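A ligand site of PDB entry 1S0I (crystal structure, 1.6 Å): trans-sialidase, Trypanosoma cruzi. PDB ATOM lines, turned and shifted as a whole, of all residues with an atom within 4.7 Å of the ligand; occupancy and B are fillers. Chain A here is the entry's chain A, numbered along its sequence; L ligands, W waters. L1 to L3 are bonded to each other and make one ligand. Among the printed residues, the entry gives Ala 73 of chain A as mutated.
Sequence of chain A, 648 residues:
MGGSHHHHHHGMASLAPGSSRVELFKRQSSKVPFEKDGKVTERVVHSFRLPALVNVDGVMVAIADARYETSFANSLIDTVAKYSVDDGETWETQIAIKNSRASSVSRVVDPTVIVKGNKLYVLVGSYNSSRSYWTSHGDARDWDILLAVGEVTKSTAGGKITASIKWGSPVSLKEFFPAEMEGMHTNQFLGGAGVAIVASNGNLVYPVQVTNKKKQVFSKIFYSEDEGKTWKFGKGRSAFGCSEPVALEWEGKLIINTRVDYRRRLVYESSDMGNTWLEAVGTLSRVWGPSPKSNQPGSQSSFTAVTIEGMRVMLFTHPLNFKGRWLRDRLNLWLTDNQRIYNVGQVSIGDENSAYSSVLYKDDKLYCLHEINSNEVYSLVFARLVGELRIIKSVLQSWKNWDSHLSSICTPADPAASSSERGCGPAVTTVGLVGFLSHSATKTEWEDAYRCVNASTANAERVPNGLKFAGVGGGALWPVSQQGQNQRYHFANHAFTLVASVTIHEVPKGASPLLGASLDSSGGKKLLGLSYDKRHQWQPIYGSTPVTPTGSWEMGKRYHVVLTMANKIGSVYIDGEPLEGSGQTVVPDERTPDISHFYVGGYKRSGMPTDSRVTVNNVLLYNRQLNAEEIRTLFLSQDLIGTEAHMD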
ATOM      1  N   ARG A  49     -15.447  34.134 -19.272  1.00  0.00           N
ATOM      2  CA  ARG A  49     -15.153  32.845 -19.912  1.00  0.00           C
ATOM      3  C   ARG A  49     -14.003  32.989 -20.913  1.00  0.00           C
ATOM      4  O   ARG A  49     -13.482  34.075 -21.115  1.00  0.00           O
ATOM      5  CB  ARG A  49     -16.400  32.364 -20.675  1.00  0.00           C
ATOM      6  CG  ARG A  49     -17.538  31.914 -19.747  1.00  0.00           C
ATOM      7  CD  ARG A  49     -18.404  30.801 -20.346  1.00  0.00           C
ATOM      8  NE  ARG A  49     -17.529  29.663 -20.678  1.00  0.00           N
ATOM      9  CZ  ARG A  49     -17.845  28.682 -21.498  1.00  0.00           C
ATOM     10  NH1 ARG A  49     -16.965  27.708 -21.700  1.00  0.00           N
ATOM     11  NH2 ARG A  49     -19.055  28.614 -22.061  1.00  0.00           N
ATOM     12  N   LEU A  50     -13.585  31.881 -21.497  1.00  0.00           N
ATOM     13  CA  LEU A  50     -12.644  31.908 -22.641  1.00  0.00           C
ATOM     14  C   LEU A  50     -11.275  32.432 -22.219  1.00  0.00           C
ATOM     15  O   LEU A  50     -10.695  33.349 -22.836  1.00  0.00           O
ATOM     16  CB  LEU A  50     -13.215  32.691 -23.839  1.00  0.00           C
ATOM     17  CG  LEU A  50     -14.112  31.926 -24.834  1.00  0.00           C
ATOM     18  CD1 LEU A  50     -13.226  31.113 -25.780  1.00  0.00           C
ATOM     19  CD2 LEU A  50     -15.116  31.016 -24.118  1.00  0.00           C
ATOM     20  N   ARG A  67     -18.828  38.669 -20.258  1.00  0.00           N
ATOM     21  CA  ARG A  67     -20.224  38.447 -20.647  1.00  0.00           C
ATOM     22  C   ARG A  67     -21.037  39.223 -19.619  1.00  0.00           C
ATOM     23  O   ARG A  67     -21.278  38.780 -18.479  1.00  0.00           O
ATOM     24  CB  ARG A  67     -20.565  36.956 -20.662  1.00  0.00           C
ATOM     25  CG  ARG A  67     -19.538  36.108 -21.475  1.00  0.00           C
ATOM     26  CD  ARG A  67     -20.109  34.795 -21.910  1.00  0.00           C
ATOM     27  NE  ARG A  67     -19.126  34.077 -22.738  1.00  0.00           N
ATOM     28  CZ  ARG A  67     -19.360  32.901 -23.265  1.00  0.00           C
ATOM     29  NH1 ARG A  67     -20.545  32.310 -23.079  1.00  0.00           N
ATOM     30  NH2 ARG A  67     -18.413  32.347 -24.040  1.00  0.00           N
ATOM     31  N   SER A  71     -24.321  34.266 -19.034  1.00  0.00           N
ATOM     32  CA  SER A  71     -23.257  33.444 -19.621  1.00  0.00           C
ATOM     33  C   SER A  71     -23.707  32.844 -20.954  1.00  0.00           C
ATOM     34  O   SER A  71     -22.887  32.214 -21.632  1.00  0.00           O
ATOM     35  CB  SER A  71     -22.879  32.330 -18.678  1.00  0.00           C
ATOM     36  OG  SER A  71     -24.023  31.532 -18.432  1.00  0.00           O
ATOM     37  N   ALA A  73     -24.202  32.166 -24.666  1.00  0.00           N
ATOM     38  CA  ALA A  73     -23.233  32.526 -25.685  1.00  0.00           C
ATOM     39  C   ALA A  73     -23.620  33.772 -26.513  1.00  0.00           C
ATOM     40  O   ALA A  73     -22.767  34.560 -26.948  1.00  0.00           O
ATOM     41  CB  ALA A  73     -23.051  31.339 -26.638  1.00  0.00           C
ATOM     42  N   VAL A 109     -16.349  37.525 -29.871  1.00  0.00           N
ATOM     43  CA  VAL A 109     -16.365  36.218 -29.233  1.00  0.00           C
ATOM     44  C   VAL A 109     -15.124  35.358 -29.437  1.00  0.00           C
ATOM     45  O   VAL A 109     -14.415  35.492 -30.445  1.00  0.00           O
ATOM     46  CB  VAL A 109     -17.562  35.380 -29.740  1.00  0.00           C
ATOM     47  CG1 VAL A 109     -18.872  36.106 -29.472  1.00  0.00           C
ATOM     48  CG2 VAL A 109     -17.439  35.077 -31.216  1.00  0.00           C
ATOM     49  N   ASP A 110     -14.913  34.475 -28.465  1.00  0.00           N
ATOM     50  CA  ASP A 110     -13.895  33.430 -28.508  1.00  0.00           C
ATOM     51  C   ASP A 110     -12.522  33.940 -28.907  1.00  0.00           C
ATOM     52  O   ASP A 110     -11.897  33.449 -29.857  1.00  0.00           O
ATOM     53  CB  ASP A 110     -14.361  32.291 -29.429  1.00  0.00           C
ATOM     54  CG  ASP A 110     -15.615  31.596 -28.865  1.00  0.00           C
ATOM     55  OD1 ASP A 110     -16.177  30.702 -29.557  1.00  0.00           O
ATOM     56  OD2 ASP A 110     -16.095  31.892 -27.735  1.00  0.00           O
ATOM     57  N   TYR A 133     -26.896  30.022 -32.050  1.00  0.00           N
ATOM     58  CA  TYR A 133     -25.504  29.540 -32.025  1.00  0.00           C
ATOM     59  C   TYR A 133     -24.914  29.580 -33.428  1.00  0.00           C
ATOM     60  O   TYR A 133     -25.584  29.297 -34.418  1.00  0.00           O
ATOM     61  CB  TYR A 133     -25.433  28.138 -31.427  1.00  0.00           C
ATOM     62  CG  TYR A 133     -25.746  28.130 -29.967  1.00  0.00           C
ATOM     63  CD1 TYR A 133     -27.003  27.764 -29.499  1.00  0.00           C
ATOM     64  CD2 TYR A 133     -24.778  28.533 -29.032  1.00  0.00           C
ATOM     65  CE1 TYR A 133     -27.272  27.778 -28.147  1.00  0.00           C
ATOM     66  CE2 TYR A 133     -25.051  28.518 -27.669  1.00  0.00           C
ATOM     67  CZ  TYR A 133     -26.295  28.165 -27.259  1.00  0.00           C
ATOM     68  OH  TYR A 133     -26.604  28.156 -25.891  1.00  0.00           O
ATOM     69  N   TRP A 134     -23.642  29.929 -33.509  1.00  0.00           N
ATOM     70  CA  TRP A 134     -23.068  30.236 -34.812  1.00  0.00           C
ATOM     71  C   TRP A 134     -23.142  29.136 -35.852  1.00  0.00           C
ATOM     72  O   TRP A 134     -23.327  29.417 -37.033  1.00  0.00           O
ATOM     73  CB  TRP A 134     -21.657  30.776 -34.624  1.00  0.00           C
ATOM     74  CG  TRP A 134     -20.576  29.704 -34.371  1.00  0.00           C
ATOM     75  CD1 TRP A 134     -20.418  28.946 -33.254  1.00  0.00           C
ATOM     76  CD2 TRP A 134     -19.517  29.364 -35.261  1.00  0.00           C
ATOM     77  NE1 TRP A 134     -19.304  28.138 -33.393  1.00  0.00           N
ATOM     78  CE2 TRP A 134     -18.752  28.368 -34.638  1.00  0.00           C
ATOM     79  CE3 TRP A 134     -19.166  29.777 -36.552  1.00  0.00           C
ATOM     80  CZ2 TRP A 134     -17.608  27.790 -35.225  1.00  0.00           C
ATOM     81  CZ3 TRP A 134     -18.038  29.205 -37.149  1.00  0.00           C
ATOM     82  CH2 TRP A 134     -17.271  28.217 -36.482  1.00  0.00           C
ATOM     83  N   THR A 135     -22.998  27.866 -35.455  1.00  0.00           N
ATOM     84  CA  THR A 135     -22.998  26.823 -36.489  1.00  0.00           C
ATOM     85  C   THR A 135     -24.404  26.536 -36.982  1.00  0.00           C
ATOM     86  O   THR A 135     -24.597  25.790 -37.945  1.00  0.00           O
ATOM     87  CB  THR A 135     -22.304  25.524 -36.045  1.00  0.00           C
ATOM     88  OG1 THR A 135     -23.060  24.934 -34.966  1.00  0.00           O
ATOM     89  CG2 THR A 135     -20.920  25.833 -35.500  1.00  0.00           C
ATOM     90  N   LEU A 190     -14.077  31.281 -37.001  1.00  0.00           N
ATOM     91  CA  LEU A 190     -13.606  31.814 -35.724  1.00  0.00           C
ATOM     92  C   LEU A 190     -12.249  31.273 -35.397  1.00  0.00           C
ATOM     93  O   LEU A 190     -11.836  30.227 -35.917  1.00  0.00           O
ATOM     94  CB  LEU A 190     -14.554  31.393 -34.588  1.00  0.00           C
ATOM     95  CG  LEU A 190     -16.011  31.776 -34.726  1.00  0.00           C
ATOM     96  CD1 LEU A 190     -16.751  31.144 -33.552  1.00  0.00           C
ATOM     97  CD2 LEU A 190     -16.144  33.292 -34.723  1.00  0.00           C
ATOM     98  N   SER A 243     -13.843  21.044 -34.117  1.00  0.00           N
ATOM     99  CA  SER A 243     -13.976  22.481 -33.823  1.00  0.00           C
ATOM    100  C   SER A 243     -12.895  22.882 -32.815  1.00  0.00           C
ATOM    101  O   SER A 243     -12.043  22.053 -32.460  1.00  0.00           O
ATOM    102  CB  SER A 243     -15.392  22.740 -33.259  1.00  0.00           C
ATOM    103  OG  SER A 243     -15.467  22.043 -32.010  1.00  0.00           O
ATOM    104  N   GLU A 244     -12.912  24.126 -32.354  1.00  0.00           N
ATOM    105  CA  GLU A 244     -11.913  24.654 -31.400  1.00  0.00           C
ATOM    106  C   GLU A 244     -10.533  24.036 -31.498  1.00  0.00           C
ATOM    107  O   GLU A 244     -10.018  23.477 -30.514  1.00  0.00           O
ATOM    108  CB  GLU A 244     -12.437  24.580 -29.966  1.00  0.00           C
ATOM    109  CG  GLU A 244     -13.502  25.644 -29.742  1.00  0.00           C
ATOM    110  CD  GLU A 244     -14.068  25.613 -28.356  1.00  0.00           C
ATOM    111  OE1 GLU A 244     -13.850  24.603 -27.618  1.00  0.00           O
ATOM    112  OE2 GLU A 244     -14.765  26.612 -28.018  1.00  0.00           O
ATOM    113  N   ARG A 259     -11.187  19.663 -30.825  1.00  0.00           N
ATOM    114  CA  ARG A 259     -12.409  19.301 -30.122  1.00  0.00           C
ATOM    115  C   ARG A 259     -13.333  18.558 -31.079  1.00  0.00           C
ATOM    116  O   ARG A 259     -13.614  19.044 -32.201  1.00  0.00           O
ATOM    117  CB  ARG A 259     -13.094  20.569 -29.626  1.00  0.00           C
ATOM    118  CG  ARG A 259     -14.494  20.335 -29.019  1.00  0.00           C
ATOM    119  CD  ARG A 259     -14.989  21.655 -28.406  1.00  0.00           C
ATOM    120  NE  ARG A 259     -16.399  21.540 -28.029  1.00  0.00           N
ATOM    121  CZ  ARG A 259     -17.018  22.495 -27.347  1.00  0.00           C
ATOM    122  NH1 ARG A 259     -16.367  23.568 -26.962  1.00  0.00           N
ATOM    123  NH2 ARG A 259     -18.322  22.366 -27.060  1.00  0.00           N
ATOM    124  N   ARG A 325     -22.832  16.481 -20.380  1.00  0.00           N
ATOM    125  CA  ARG A 325     -23.263  17.710 -21.033  1.00  0.00           C
ATOM    126  C   ARG A 325     -22.114  18.695 -21.054  1.00  0.00           C
ATOM    127  O   ARG A 325     -20.964  18.299 -21.332  1.00  0.00           O
ATOM    128  CB  ARG A 325     -24.540  18.232 -20.372  1.00  0.00           C
ATOM    129  CG  ARG A 325     -25.690  17.276 -20.715  1.00  0.00           C
ATOM    130  CD  ARG A 325     -27.035  17.695 -20.097  1.00  0.00           C
ATOM    131  NE  ARG A 325     -27.495  18.959 -20.660  1.00  0.00           N
ATOM    132  CZ  ARG A 325     -28.107  19.099 -21.843  1.00  0.00           C
ATOM    133  NH1 ARG A 325     -28.352  18.030 -22.607  1.00  0.00           N
ATOM    134  NH2 ARG A 325     -28.466  20.306 -22.257  1.00  0.00           N
ATOM    135  N   TRP A 326     -22.385  19.966 -20.782  1.00  0.00           N
ATOM    136  CA  TRP A 326     -21.334  20.959 -20.812  1.00  0.00           C
ATOM    137  C   TRP A 326     -20.784  21.274 -19.443  1.00  0.00           C
ATOM    138  O   TRP A 326     -19.962  22.194 -19.282  1.00  0.00           O
ATOM    139  CB  TRP A 326     -21.828  22.253 -21.508  1.00  0.00           C
ATOM    140  CG  TRP A 326     -22.036  22.051 -23.015  1.00  0.00           C
ATOM    141  CD1 TRP A 326     -21.133  22.343 -24.021  1.00  0.00           C
ATOM    142  CD2 TRP A 326     -23.175  21.481 -23.659  1.00  0.00           C
ATOM    143  NE1 TRP A 326     -21.676  22.002 -25.248  1.00  0.00           N
ATOM    144  CE2 TRP A 326     -22.929  21.480 -25.049  1.00  0.00           C
ATOM    145  CE3 TRP A 326     -24.411  20.998 -23.214  1.00  0.00           C
ATOM    146  CZ2 TRP A 326     -23.845  20.994 -25.998  1.00  0.00           C
ATOM    147  CZ3 TRP A 326     -25.331  20.515 -24.153  1.00  0.00           C
ATOM    148  CH2 TRP A 326     -25.043  20.520 -25.529  1.00  0.00           C
ATOM    149  N   ARG A 328     -18.573  19.695 -17.491  1.00  0.00           N
ATOM    150  CA  ARG A 328     -17.123  19.665 -17.683  1.00  0.00           C
ATOM    151  C   ARG A 328     -16.293  19.915 -16.425  1.00  0.00           C
ATOM    152  O   ARG A 328     -15.408  20.748 -16.363  1.00  0.00           O
ATOM    153  CB  ARG A 328     -16.771  20.600 -18.860  1.00  0.00           C
ATOM    154  CG  ARG A 328     -17.262  19.944 -20.174  1.00  0.00           C
ATOM    155  CD  ARG A 328     -17.123  20.804 -21.420  1.00  0.00           C
ATOM    156  NE  ARG A 328     -17.873  22.041 -21.230  1.00  0.00           N
ATOM    157  CZ  ARG A 328     -17.986  22.994 -22.144  1.00  0.00           C
ATOM    158  NH1 ARG A 328     -17.409  22.861 -23.349  1.00  0.00           N
ATOM    159  NH2 ARG A 328     -18.675  24.086 -21.830  1.00  0.00           N
ATOM    160  N   TYR A 356     -12.908  25.508 -19.612  1.00  0.00           N
ATOM    161  CA  TYR A 356     -11.836  26.093 -20.427  1.00  0.00           C
ATOM    162  C   TYR A 356     -10.640  26.526 -19.583  1.00  0.00           C
ATOM    163  O   TYR A 356     -10.782  26.847 -18.403  1.00  0.00           O
ATOM    164  CB  TYR A 356     -12.382  27.287 -21.218  1.00  0.00           C
ATOM    165  CG  TYR A 356     -13.274  26.909 -22.378  1.00  0.00           C
ATOM    166  CD1 TYR A 356     -14.055  25.746 -22.394  1.00  0.00           C
ATOM    167  CD2 TYR A 356     -13.384  27.778 -23.452  1.00  0.00           C
ATOM    168  CE1 TYR A 356     -14.902  25.455 -23.478  1.00  0.00           C
ATOM    169  CE2 TYR A 356     -14.185  27.510 -24.539  1.00  0.00           C
ATOM    170  CZ  TYR A 356     -14.950  26.362 -24.555  1.00  0.00           C
ATOM    171  OH  TYR A 356     -15.744  26.108 -25.668  1.00  0.00           O
ATOM    172  N   GLU A 376     -24.176  28.143 -14.070  1.00  0.00           N
ATOM    173  CA  GLU A 376     -23.979  28.925 -15.294  1.00  0.00           C
ATOM    174  C   GLU A 376     -23.557  30.383 -15.019  1.00  0.00           C
ATOM    175  O   GLU A 376     -23.855  31.289 -15.780  1.00  0.00           O
ATOM    176  CB  GLU A 376     -25.174  28.788 -16.264  1.00  0.00           C
ATOM    177  CG  GLU A 376     -25.472  27.352 -16.683  1.00  0.00           C
ATOM    178  CD  GLU A 376     -24.234  26.669 -17.244  1.00  0.00           C
ATOM    179  OE1 GLU A 376     -23.603  27.271 -18.136  1.00  0.00           O
ATOM    180  OE2 GLU A 376     -23.900  25.562 -16.789  1.00  0.00           O
ATOM    181  N   TYR A 378     -19.936  32.083 -14.363  1.00  0.00           N
ATOM    182  CA  TYR A 378     -18.539  31.703 -14.520  1.00  0.00           C
ATOM    183  C   TYR A 378     -17.523  32.735 -14.022  1.00  0.00           C
ATOM    184  O   TYR A 378     -17.608  33.936 -14.353  1.00  0.00           O
ATOM    185  CB  TYR A 378     -18.231  31.490 -16.015  1.00  0.00           C
ATOM    186  CG  TYR A 378     -18.997  30.382 -16.726  1.00  0.00           C
ATOM    187  CD1 TYR A 378     -20.371  30.496 -16.934  1.00  0.00           C
ATOM    188  CD2 TYR A 378     -18.345  29.250 -17.189  1.00  0.00           C
ATOM    189  CE1 TYR A 378     -21.081  29.505 -17.613  1.00  0.00           C
ATOM    190  CE2 TYR A 378     -19.040  28.256 -17.895  1.00  0.00           C
ATOM    191  CZ  TYR A 378     -20.392  28.366 -18.081  1.00  0.00           C
ATOM    192  OH  TYR A 378     -21.101  27.400 -18.746  1.00  0.00           O
HETATM  193  C1  LIG L   1     -28.276  23.263 -26.323  1.00  0.00           C
HETATM  194  C2  LIG L   1     -27.723  23.339 -24.908  1.00  0.00           C
HETATM  195  C3  LIG L   1     -26.719  24.452 -24.765  1.00  0.00           C
HETATM  196  C4  LIG L   1     -25.634  24.230 -25.823  1.00  0.00           C
HETATM  197  C5  LIG L   1     -26.247  24.112 -27.198  1.00  0.00           C
HETATM  198  C6  LIG L   1     -25.221  23.682 -28.251  1.00  0.00           C
HETATM  199  O1  LIG L   1     -28.869  24.492 -26.671  1.00  0.00           O
HETATM  200  O2  LIG L   1     -28.795  23.611 -23.995  1.00  0.00           O
HETATM  201  O3  LIG L   1     -26.157  24.388 -23.449  1.00  0.00           O
HETATM  202  O4  LIG L   1     -24.813  25.381 -25.925  1.00  0.00           O
HETATM  203  O5  LIG L   1     -27.182  23.045 -27.204  1.00  0.00           O
HETATM  204  O6  LIG L   1     -24.402  24.774 -28.702  1.00  0.00           O
HETATM  205  C1  LG2 L   2     -23.619  25.379 -25.163  1.00  0.00           C
HETATM  206  C2  LG2 L   2     -22.630  26.304 -25.845  1.00  0.00           C
HETATM  207  C3  LG2 L   2     -21.360  26.422 -24.998  1.00  0.00           C
HETATM  208  C4  LG2 L   2     -21.738  26.808 -23.572  1.00  0.00           C
HETATM  209  C5  LG2 L   2     -22.824  25.887 -23.015  1.00  0.00           C
HETATM  210  C6  LG2 L   2     -23.248  26.312 -21.613  1.00  0.00           C
HETATM  211  O1  LG2 L   2     -22.312  25.704 -27.099  1.00  0.00           O
HETATM  212  O2  LG2 L   2     -20.427  27.370 -25.503  1.00  0.00           O
HETATM  213  O3  LG2 L   2     -22.203  28.157 -23.590  1.00  0.00           O
HETATM  214  O4  LG2 L   2     -23.925  25.877 -23.884  1.00  0.00           O
HETATM  215  O5  LG2 L   2     -24.109  25.279 -21.135  1.00  0.00           O
HETATM  216  C1  LG3 L   3     -18.681  25.899 -24.821  1.00  0.00           C
HETATM  217  C2  LG3 L   3     -19.077  26.993 -25.786  1.00  0.00           C
HETATM  218  C3  LG3 L   3     -18.129  28.164 -25.552  1.00  0.00           C
HETATM  219  C4  LG3 L   3     -17.914  29.098 -26.763  1.00  0.00           C
HETATM  220  C5  LG3 L   3     -18.908  28.772 -27.859  1.00  0.00           C
HETATM  221  C6  LG3 L   3     -18.779  27.279 -28.201  1.00  0.00           C
HETATM  222  C7  LG3 L   3     -19.719  26.812 -29.307  1.00  0.00           C
HETATM  223  C8  LG3 L   3     -19.621  25.324 -29.548  1.00  0.00           C
HETATM  224  C9  LG3 L   3     -20.624  24.926 -30.629  1.00  0.00           C
HETATM  225  C10 LG3 L   3     -19.673  30.122 -29.756  1.00  0.00           C
HETATM  226  C11 LG3 L   3     -19.277  31.137 -30.796  1.00  0.00           C
HETATM  227  N1  LG3 L   3     -18.677  29.614 -29.046  1.00  0.00           N
HETATM  228  O1  LG3 L   3     -18.585  26.195 -23.612  1.00  0.00           O
HETATM  229  O2  LG3 L   3     -18.528  24.715 -25.192  1.00  0.00           O
HETATM  230  O3  LG3 L   3     -18.169  30.440 -26.350  1.00  0.00           O
HETATM  231  O4  LG3 L   3     -19.001  26.442 -27.070  1.00  0.00           O
HETATM  232  O5  LG3 L   3     -21.073  27.139 -29.004  1.00  0.00           O
HETATM  233  O6  LG3 L   3     -18.270  24.996 -29.910  1.00  0.00           O
HETATM  234  O7  LG3 L   3     -20.321  25.571 -31.888  1.00  0.00           O
HETATM  235  O8  LG3 L   3     -20.865  29.836 -29.634  1.00  0.00           O
HETATM  236  O   HOH W   1     -26.927  20.801 -28.863  1.00  0.00           O
HETATM  237  O   HOH W   2     -20.746  30.199 -24.975  1.00  0.00           O
HETATM  238  O   HOH W   3     -22.720  31.206 -31.007  1.00  0.00           O
HETATM  239  O   HOH W   4     -22.736  26.444 -32.793  1.00  0.00           O
HETATM  240  O   HOH W   5     -17.178  26.741 -31.649  1.00  0.00           O
HETATM  241  O   HOH W   6     -21.287  23.073 -27.787  1.00  0.00           O
HETATM  242  O   HOH W   7     -24.401  24.820 -31.430  1.00  0.00           O
HETATM  243  O   HOH W   8     -21.808  29.621 -21.379  1.00  0.00           O
HETATM  244  O   HOH W   9     -22.988  24.009 -18.912  1.00  0.00           O
HETATM  245  O   HOH W  10     -26.635  26.351 -20.690  1.00  0.00           O
HETATM  246  O   HOH W  11     -26.609  22.833 -21.125  1.00  0.00           O
HETATM  247  O   HOH W  12     -24.748  29.224 -24.213  1.00  0.00           O
HETATM  248  O   HOH W  13     -29.002  25.896 -22.544  1.00  0.00           O
HETATM  249  O   HOH W  14     -30.768  21.915 -23.735  1.00  0.00           O
HETATM  250  O   HOH W  15     -17.929  22.465 -30.895  1.00  0.00           O
HETATM  251  O   HOH W  16     -18.928  23.674 -33.286  1.00  0.00           O
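OH of Tyr 356 lies close to O2 of LG3 L3 (3.1 Å).
NH2 of Arg 49 is in salt-bridge range of O1 of LG3 L3.
N1 of LG3 L3 lies within hydrogen-bond range of OD1 of Asp 110 (2.8 Å).
O1 of LG3 L3 lies within salt-bridge range of NH2 of Arg 328, at 2.8 Å.
OH of Tyr 133 is in hydrogen-bond range of O4 of LIG L1.
O3 of LG3 L3 is in hydrogen-bond range of NH2 of Arg 67, 3.0 Å away.
The guanidinium group (NH2) of Arg 259 lies within salt-bridge range of an oxygen (O2) of LG3 L3 (3.0 Å).
NE1 of Trp 134 sits at hydrogen-bond distance from O7 of LG3 L3 (3.1 Å).
Water W14 bridges O2 of LIG L1 (2.6 Å) and NH2 of Arg 325 (3.2 Å).
Water W8 lies within hydrogen-bond range of an oxygen (O3) of LG2 L2 (2.7 Å), the backbone carbonyl oxygen (O) of Ser 71 (2.8 Å), the guanidinium group (NH2) of Arg 49 (3.0 Å) and the guanidinium group (NH1) of Arg 67 (3.4 Å).
Water W4 bridges OG1 of Thr 135 and O7 of LG3 L3.
Water W15 lies within hydrogen-bond range of OG of Ser 243, O6 of LG3 L3 and NE of Arg 259.
Water W12 lies within hydrogen-bond range of the side-chain hydroxyl of Tyr 133 (2.7 Å), an oxygen (O3) of LG2 L2 (2.8 Å) and the backbone NH of Ala 73 (3.0 Å).
Water W2 bridges the guanidinium group (NH1) of Arg 67 (2.8 Å) and an oxygen (O3) of LG2 L2 (2.9 Å).
Residues that only touch the ligand: Leu 50, Thr 135, Leu 190, Arg 325, Trp 326, Glu 376 and Tyr 378.
Hydrophobic or aromatic side chains that line the ligand: Leu 50, Tyr 133, Trp 134, Leu 190, Trp 326 and Tyr 356.
15 residues have an atom within 4 Å of the ligand: Arg 49, Leu 50, Arg 67, Asp 110, Tyr 133, Trp 134, Thr 135, Leu 190, Arg 259, Arg 325, Trp 326, Arg 328, Tyr 356, Glu 376 and Tyr 378.
The guanidinium group (NH1) of Arg 67 sits at hydrogen-bond distance from the backbone carbonyl oxygen (O) of Ser 71, 2.8 Å away.
The side-chain hydroxyl of Tyr 356 sits at hydrogen-bond distance from the guanidinium group of Arg 259 (2.9 Å).
OH of Tyr 356 is in hydrogen-bond range of OE2 of Glu 244, at 2.6 Å.
The backbone carbonyl oxygen (O) of Glu 376 is in hydrogen-bond range of the side-chain hydroxyl (OG) of Ser 71, at 2.7 Å.
The guanidinium group of Arg 328 sits at hydrogen-bond distance from the backbone carbonyl oxygen of Trp 326, at 2.9 Å.
The side-chain carboxylate (OE1) of Glu 244 is in salt-bridge range of the guanidinium group (NH1) of Arg 259, 2.8 Å away.
O of Arg 259 sits at hydrogen-bond distance from N of Ser 243, at 2.8 Å.
The side-chain hydroxyl (OH) of Tyr 378 lies within hydrogen-bond range of the side-chain carboxylate (OE1) of Glu 376, 2.6 Å away.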
